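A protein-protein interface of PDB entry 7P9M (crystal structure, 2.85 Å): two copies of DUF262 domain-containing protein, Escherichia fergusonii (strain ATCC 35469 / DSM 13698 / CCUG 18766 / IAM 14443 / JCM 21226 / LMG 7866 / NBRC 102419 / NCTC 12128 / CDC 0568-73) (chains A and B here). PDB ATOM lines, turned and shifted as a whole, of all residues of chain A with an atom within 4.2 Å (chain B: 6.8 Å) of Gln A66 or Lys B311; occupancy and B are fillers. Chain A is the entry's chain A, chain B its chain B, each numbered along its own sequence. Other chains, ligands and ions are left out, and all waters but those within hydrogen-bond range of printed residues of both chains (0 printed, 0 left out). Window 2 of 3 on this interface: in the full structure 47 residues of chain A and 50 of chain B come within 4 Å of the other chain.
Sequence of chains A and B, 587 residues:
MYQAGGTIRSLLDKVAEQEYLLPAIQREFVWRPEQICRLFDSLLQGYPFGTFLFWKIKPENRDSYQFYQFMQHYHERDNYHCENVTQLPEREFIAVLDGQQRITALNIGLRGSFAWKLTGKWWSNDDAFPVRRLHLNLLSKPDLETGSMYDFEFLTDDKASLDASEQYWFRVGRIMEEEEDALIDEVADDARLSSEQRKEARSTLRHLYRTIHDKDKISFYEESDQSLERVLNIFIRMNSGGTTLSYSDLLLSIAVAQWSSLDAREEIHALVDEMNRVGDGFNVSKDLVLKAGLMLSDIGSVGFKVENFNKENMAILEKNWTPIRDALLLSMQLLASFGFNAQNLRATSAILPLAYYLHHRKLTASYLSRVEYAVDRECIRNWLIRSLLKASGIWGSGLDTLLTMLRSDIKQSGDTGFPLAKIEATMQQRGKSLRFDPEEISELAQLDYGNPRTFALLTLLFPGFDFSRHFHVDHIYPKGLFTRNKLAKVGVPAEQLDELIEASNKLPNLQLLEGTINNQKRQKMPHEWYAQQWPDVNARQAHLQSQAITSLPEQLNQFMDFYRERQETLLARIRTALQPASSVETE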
ATOM      1  N   PRO A  23      13.957   1.741  11.755  1.00  0.00           N
ATOM      2  CA  PRO A  23      13.462   2.958  11.143  1.00  0.00           C
ATOM      3  C   PRO A  23      12.153   3.415  11.778  1.00  0.00           C
ATOM      4  O   PRO A  23      12.001   4.585  11.953  1.00  0.00           O
ATOM      5  CB  PRO A  23      13.195   2.584   9.686  1.00  0.00           C
ATOM      6  CG  PRO A  23      12.880   1.123   9.708  1.00  0.00           C
ATOM      7  CD  PRO A  23      13.725   0.600  10.842  1.00  0.00           C
ATOM      8  N   SER A  64      19.278  11.712   7.750  1.00  0.00           N
ATOM      9  CA  SER A  64      18.092  12.012   6.913  1.00  0.00           C
ATOM     10  C   SER A  64      16.854  11.169   7.195  1.00  0.00           C
ATOM     11  O   SER A  64      15.890  11.368   6.473  1.00  0.00           O
ATOM     12  CB  SER A  64      18.458  11.881   5.481  1.00  0.00           C
ATOM     13  OG  SER A  64      18.814  10.542   5.178  1.00  0.00           O
ATOM     14  N   TYR A  65      16.856  10.248   8.174  1.00  0.00           N
ATOM     15  CA  TYR A  65      15.664   9.357   8.312  1.00  0.00           C
ATOM     16  C   TYR A  65      15.201   9.078   9.750  1.00  0.00           C
ATOM     17  O   TYR A  65      14.318   8.206   9.861  1.00  0.00           O
ATOM     18  CB  TYR A  65      15.892   8.000   7.639  1.00  0.00           C
ATOM     19  CG  TYR A  65      16.101   8.021   6.147  1.00  0.00           C
ATOM     20  CD1 TYR A  65      15.028   8.109   5.276  1.00  0.00           C
ATOM     21  CD2 TYR A  65      17.372   7.934   5.606  1.00  0.00           C
ATOM     22  CE1 TYR A  65      15.215   8.122   3.905  1.00  0.00           C
ATOM     23  CE2 TYR A  65      17.577   7.948   4.237  1.00  0.00           C
ATOM     24  CZ  TYR A  65      16.493   8.042   3.384  1.00  0.00           C
ATOM     25  OH  TYR A  65      16.690   8.054   2.035  1.00  0.00           O
ATOM     26  N   GLN A  66      15.754   9.728  10.781  1.00  0.00           N
ATOM     27  CA  GLN A  66      15.257   9.572  12.184  1.00  0.00           C
ATOM     28  C   GLN A  66      15.123   8.156  12.771  1.00  0.00           C
ATOM     29  O   GLN A  66      14.014   7.817  13.237  1.00  0.00           O
ATOM     30  CB  GLN A  66      13.903  10.267  12.353  1.00  0.00           C
ATOM     31  CG  GLN A  66      13.971  11.780  12.230  1.00  0.00           C
ATOM     32  CD  GLN A  66      12.615  12.433  12.329  1.00  0.00           C
ATOM     33  OE1 GLN A  66      11.590  11.822  12.039  1.00  0.00           O
ATOM     34  NE2 GLN A  66      12.605  13.685  12.752  1.00  0.00           N
ATOM     35  N   PHE A  67      16.221   7.394  12.832  1.00  0.00           N
ATOM     36  CA  PHE A  67      16.182   6.011  13.342  1.00  0.00           C
ATOM     37  C   PHE A  67      15.936   5.923  14.841  1.00  0.00           C
ATOM     38  O   PHE A  67      16.175   6.899  15.541  1.00  0.00           O
ATOM     39  CB  PHE A  67      17.478   5.349  12.896  1.00  0.00           C
ATOM     40  CG  PHE A  67      17.896   5.677  11.490  1.00  0.00           C
ATOM     41  CD1 PHE A  67      17.302   5.043  10.416  1.00  0.00           C
ATOM     42  CD2 PHE A  67      18.884   6.612  11.244  1.00  0.00           C
ATOM     43  CE1 PHE A  67      17.688   5.342   9.122  1.00  0.00           C
ATOM     44  CE2 PHE A  67      19.266   6.912   9.949  1.00  0.00           C
ATOM     45  CZ  PHE A  67      18.673   6.272   8.892  1.00  0.00           C
ATOM     46  N   TYR A  68      15.422   4.791  15.297  1.00  0.00           N
ATOM     47  CA  TYR A  68      15.096   4.622  16.727  1.00  0.00           C
ATOM     48  C   TYR A  68      15.792   3.366  17.246  1.00  0.00           C
ATOM     49  O   TYR A  68      16.013   2.450  16.466  1.00  0.00           O
ATOM     50  CB  TYR A  68      13.585   4.490  16.922  1.00  0.00           C
ATOM     51  CG  TYR A  68      12.718   5.509  16.236  1.00  0.00           C
ATOM     52  CD1 TYR A  68      12.935   6.864  16.395  1.00  0.00           C
ATOM     53  CD2 TYR A  68      11.652   5.110  15.453  1.00  0.00           C
ATOM     54  CE1 TYR A  68      12.133   7.797  15.764  1.00  0.00           C
ATOM     55  CE2 TYR A  68      10.836   6.029  14.820  1.00  0.00           C
ATOM     56  CZ  TYR A  68      11.078   7.380  14.974  1.00  0.00           C
ATOM     57  OH  TYR A  68      10.279   8.294  14.354  1.00  0.00           O
ATOM     58  N   VAL B 256       6.149   7.209   7.506  1.00  0.00           N
ATOM     59  CA  VAL B 256       5.377   7.649   8.694  1.00  0.00           C
ATOM     60  C   VAL B 256       6.352   7.894   9.830  1.00  0.00           C
ATOM     61  O   VAL B 256       6.042   8.682  10.733  1.00  0.00           O
ATOM     62  CB  VAL B 256       4.400   6.519   9.022  1.00  0.00           C
ATOM     63  CG1 VAL B 256       3.592   6.729  10.291  1.00  0.00           C
ATOM     64  CG2 VAL B 256       3.515   6.209   7.833  1.00  0.00           C
ATOM     65  N   ALA B 257       7.536   7.315   9.726  1.00  0.00           N
ATOM     66  CA  ALA B 257       8.506   7.409  10.835  1.00  0.00           C
ATOM     67  C   ALA B 257       9.343   8.671  10.723  1.00  0.00           C
ATOM     68  O   ALA B 257      10.415   8.725  11.330  1.00  0.00           O
ATOM     69  CB  ALA B 257       9.390   6.209  10.793  1.00  0.00           C
ATOM     70  N   GLN B 258       8.868   9.648   9.972  1.00  0.00           N
ATOM     71  CA  GLN B 258       9.613  10.917   9.900  1.00  0.00           C
ATOM     72  C   GLN B 258       8.632  12.048  10.188  1.00  0.00           C
ATOM     73  O   GLN B 258       8.899  13.176   9.771  1.00  0.00           O
ATOM     74  CB  GLN B 258      10.303  11.001   8.545  1.00  0.00           C
ATOM     75  CG  GLN B 258      11.597  10.215   8.463  1.00  0.00           C
ATOM     76  CD  GLN B 258      11.390   8.989   7.616  1.00  0.00           C
ATOM     77  OE1 GLN B 258      10.529   8.966   6.750  1.00  0.00           O
ATOM     78  NE2 GLN B 258      12.164   7.951   7.873  1.00  0.00           N
ATOM     79  N   TRP B 259       7.536  11.735  10.866  1.00  0.00           N
ATOM     80  CA  TRP B 259       6.485  12.750  11.107  1.00  0.00           C
ATOM     81  C   TRP B 259       6.387  13.020  12.603  1.00  0.00           C
ATOM     82  O   TRP B 259       6.646  12.094  13.374  1.00  0.00           O
ATOM     83  CB  TRP B 259       5.153  12.223  10.585  1.00  0.00           C
ATOM     84  CG  TRP B 259       4.906  12.395   9.121  1.00  0.00           C
ATOM     85  CD1 TRP B 259       5.817  12.330   8.109  1.00  0.00           C
ATOM     86  CD2 TRP B 259       3.633  12.632   8.498  1.00  0.00           C
ATOM     87  NE1 TRP B 259       5.201  12.526   6.903  1.00  0.00           N
ATOM     88  CE2 TRP B 259       3.863  12.714   7.111  1.00  0.00           C
ATOM     89  CE3 TRP B 259       2.332  12.795   8.976  1.00  0.00           C
ATOM     90  CZ2 TRP B 259       2.836  12.948   6.202  1.00  0.00           C
ATOM     91  CZ3 TRP B 259       1.316  13.025   8.079  1.00  0.00           C
ATOM     92  CH2 TRP B 259       1.568  13.101   6.712  1.00  0.00           C
ATOM     93  N   SER B 260       5.997  14.238  12.979  1.00  0.00           N
ATOM     94  CA  SER B 260       5.829  14.600  14.407  1.00  0.00           C
ATOM     95  C   SER B 260       4.639  13.832  14.957  1.00  0.00           C
ATOM     96  O   SER B 260       4.694  13.401  16.120  1.00  0.00           O
ATOM     97  CB  SER B 260       5.590  16.063  14.556  1.00  0.00           C
ATOM     98  OG  SER B 260       5.382  16.406  15.917  1.00  0.00           O
ATOM     99  N   PHE B 309      11.566   9.575   0.481  1.00  0.00           N
ATOM    100  CA  PHE B 309      10.707   9.696   1.686  1.00  0.00           C
ATOM    101  C   PHE B 309      11.578  10.067   2.883  1.00  0.00           C
ATOM    102  O   PHE B 309      11.374   9.517   3.962  1.00  0.00           O
ATOM    103  CB  PHE B 309       9.880   8.430   1.876  1.00  0.00           C
ATOM    104  CG  PHE B 309       8.816   8.219   0.829  1.00  0.00           C
ATOM    105  CD1 PHE B 309       7.557   8.767   0.977  1.00  0.00           C
ATOM    106  CD2 PHE B 309       9.072   7.473  -0.304  1.00  0.00           C
ATOM    107  CE1 PHE B 309       6.585   8.586   0.011  1.00  0.00           C
ATOM    108  CE2 PHE B 309       8.099   7.294  -1.272  1.00  0.00           C
ATOM    109  CZ  PHE B 309       6.855   7.842  -1.108  1.00  0.00           C
ATOM    110  N   ASN B 310      12.483  11.025   2.698  1.00  0.00           N
ATOM    111  CA  ASN B 310      13.427  11.419   3.770  1.00  0.00           C
ATOM    112  C   ASN B 310      12.752  12.348   4.758  1.00  0.00           C
ATOM    113  O   ASN B 310      11.624  12.715   4.520  1.00  0.00           O
ATOM    114  CB  ASN B 310      14.702  12.055   3.227  1.00  0.00           C
ATOM    115  CG  ASN B 310      14.496  13.113   2.175  1.00  0.00           C
ATOM    116  OD1 ASN B 310      14.366  14.285   2.499  1.00  0.00           O
ATOM    117  ND2 ASN B 310      14.530  12.713   0.917  1.00  0.00           N
ATOM    118  N   LYS B 311      13.471  12.769   5.791  1.00  0.00           N
ATOM    119  CA  LYS B 311      12.867  13.607   6.854  1.00  0.00           C
ATOM    120  C   LYS B 311      12.541  14.974   6.288  1.00  0.00           C
ATOM    121  O   LYS B 311      11.508  15.503   6.632  1.00  0.00           O
ATOM    122  CB  LYS B 311      13.853  13.792   8.003  1.00  0.00           C
ATOM    123  CG  LYS B 311      13.337  14.577   9.198  1.00  0.00           C
ATOM    124  CD  LYS B 311      14.382  14.705  10.277  1.00  0.00           C
ATOM    125  CE  LYS B 311      15.541  15.580   9.859  1.00  0.00           C
ATOM    126  NZ  LYS B 311      15.125  16.986   9.643  1.00  0.00           N
ATOM    127  N   GLU B 312      13.416  15.503   5.449  1.00  0.00           N
ATOM    128  CA  GLU B 312      13.185  16.858   4.919  1.00  0.00           C
ATOM    129  C   GLU B 312      11.995  16.780   3.981  1.00  0.00           C
ATOM    130  O   GLU B 312      11.156  17.666   4.017  1.00  0.00           O
ATOM    131  CB  GLU B 312      14.426  17.348   4.185  1.00  0.00           C
ATOM    132  CG  GLU B 312      15.468  17.919   5.121  1.00  0.00           C
ATOM    133  CD  GLU B 312      16.546  18.731   4.431  1.00  0.00           C
ATOM    134  OE1 GLU B 312      16.564  18.739   3.188  1.00  0.00           O
ATOM    135  OE2 GLU B 312      17.362  19.349   5.138  1.00  0.00           O
ATOM    136  N   ASN B 313      11.927  15.735   3.172  1.00  0.00           N
ATOM    137  CA  ASN B 313      10.839  15.672   2.172  1.00  0.00           C
ATOM    138  C   ASN B 313       9.517  15.476   2.908  1.00  0.00           C
ATOM    139  O   ASN B 313       8.535  16.115   2.540  1.00  0.00           O
ATOM    140  CB  ASN B 313      11.131  14.623   1.103  1.00  0.00           C
ATOM    141  CG  ASN B 313      12.178  15.057   0.103  1.00  0.00           C
ATOM    142  OD1 ASN B 313      12.791  16.107   0.257  1.00  0.00           O
ATOM    143  ND2 ASN B 313      12.392  14.249  -0.919  1.00  0.00           N
ATOM    144  N   MET B 314       9.512  14.659   3.953  1.00  0.00           N
ATOM    145  CA  MET B 314       8.239  14.341   4.641  1.00  0.00           C
ATOM    146  C   MET B 314       7.855  15.498   5.543  1.00  0.00           C
ATOM    147  O   MET B 314       6.696  15.580   5.919  1.00  0.00           O
ATOM    148  CB  MET B 314       8.371  13.076   5.482  1.00  0.00           C
ATOM    149  CG  MET B 314       8.363  11.808   4.671  1.00  0.00           C
ATOM    150  SD  MET B 314       6.806  11.619   3.802  1.00  0.00           S
ATOM    151  CE  MET B 314       7.305  12.046   2.135  1.00  0.00           C
ATOM    152  N   ALA B 315       8.804  16.359   5.857  1.00  0.00           N
ATOM    153  CA  ALA B 315       8.457  17.535   6.665  1.00  0.00           C
ATOM    154  C   ALA B 315       7.554  18.412   5.827  1.00  0.00           C
ATOM    155  O   ALA B 315       6.555  18.891   6.351  1.00  0.00           O
ATOM    156  CB  ALA B 315       9.710  18.266   6.992  1.00  0.00           C
ATOM    157  N   ILE B 316       7.882  18.569   4.553  1.00  0.00           N
ATOM    158  CA  ILE B 316       7.088  19.468   3.678  1.00  0.00           C
ATOM    159  C   ILE B 316       5.666  18.935   3.647  1.00  0.00           C
ATOM    160  O   ILE B 316       4.731  19.718   3.793  1.00  0.00           O
ATOM    161  CB  ILE B 316       7.723  19.529   2.285  1.00  0.00           C
ATOM    162  CG1 ILE B 316       9.096  20.198   2.344  1.00  0.00           C
ATOM    163  CG2 ILE B 316       6.804  20.224   1.298  1.00  0.00           C
ATOM    164  CD1 ILE B 316       9.897  20.067   1.077  1.00  0.00           C
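Among the printed residues, merely in contact across the chains: Gln A66 with Gln B258, Gln A66 with Lys B311, Pro A23 with Ala B257, Ser A64 with Asn B310 and Tyr A65 with Asn B310.
No position is printed for both chains.
Of the 9 pairs that touch across the chains among the printed residues, none has its exchanged pair printed and touching as well.
The side-chain amide oxygen (OE1) of Gln B258 sits close to the backbone carbonyl oxygen (O) of Phe B309, 3.0 Å away.
OD1 of Asn B310 sits at hydrogen-bond distance from N of Asn B313.
The backbone NH of Glu B312 sits close to the side-chain amide oxygen of Asn B310.
The backbone carbonyl oxygen of Ser A64 is in hydrogen-bond range of the backbone NH of Lys B311, 2.9 Å away.
The backbone carbonyl oxygen (O) of Tyr A65 sits at hydrogen-bond distance from the side-chain amide nitrogen (NE2) of Gln B258, 2.9 Å away.
OE1 of Gln A66 lies close to O of Ala B257, at 3.4 Å.
The side-chain hydroxyl of Tyr A68 lies within hydrogen-bond range of the backbone carbonyl oxygen of Ala B257, at 3.1 Å.
Hydrophobic or aromatic side chains of chain B that line the printed part of chain A: Ala B257.
Along chain B the printed residues that touch a printed residue of chain A span positions 257 to 311.
Of the 6 printed residues of chain A, 5 touch a printed residue of chain B.
Hydrophobic or aromatic side chains of chain A that line the printed part of chain B: Tyr A65 and Tyr A68.
Among the printed residues, 9 pairs touch across the chains.
Among the printed residues, no Asp or Glu carboxylate lies within 4 Å of a Lys or Arg side-chain nitrogen of the other chain.
Printed residues of chain B within 4 Å of Ser A64: Asn B310 (3.5 Å) and Lys B311 (2.9 Å).
Of the printed residues of chain B, Tyr A65 touches Gln B258 (2.9 Å) and Asn B310 (3.8 Å).
Of the printed residues of chain A, Ala B257 touches Pro A23, Gln A66 and Tyr A68.
Lys B311 touches just these residues of chain A: Ser A64 (2.9 Å) and Gln A66 (3.2 Å).
Ala B315 touches none of the printed residues of chain A.
The nearest residue of chain B that does not touch Gln A66 is Trp B259 (4.2 Å).
The nearest printed residue of chain A that does not touch Lys B311 is Tyr A65 (4.6 Å).
The nearest printed residue of chain B that does not touch Pro A23 is Gln B258 (5.3 Å).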
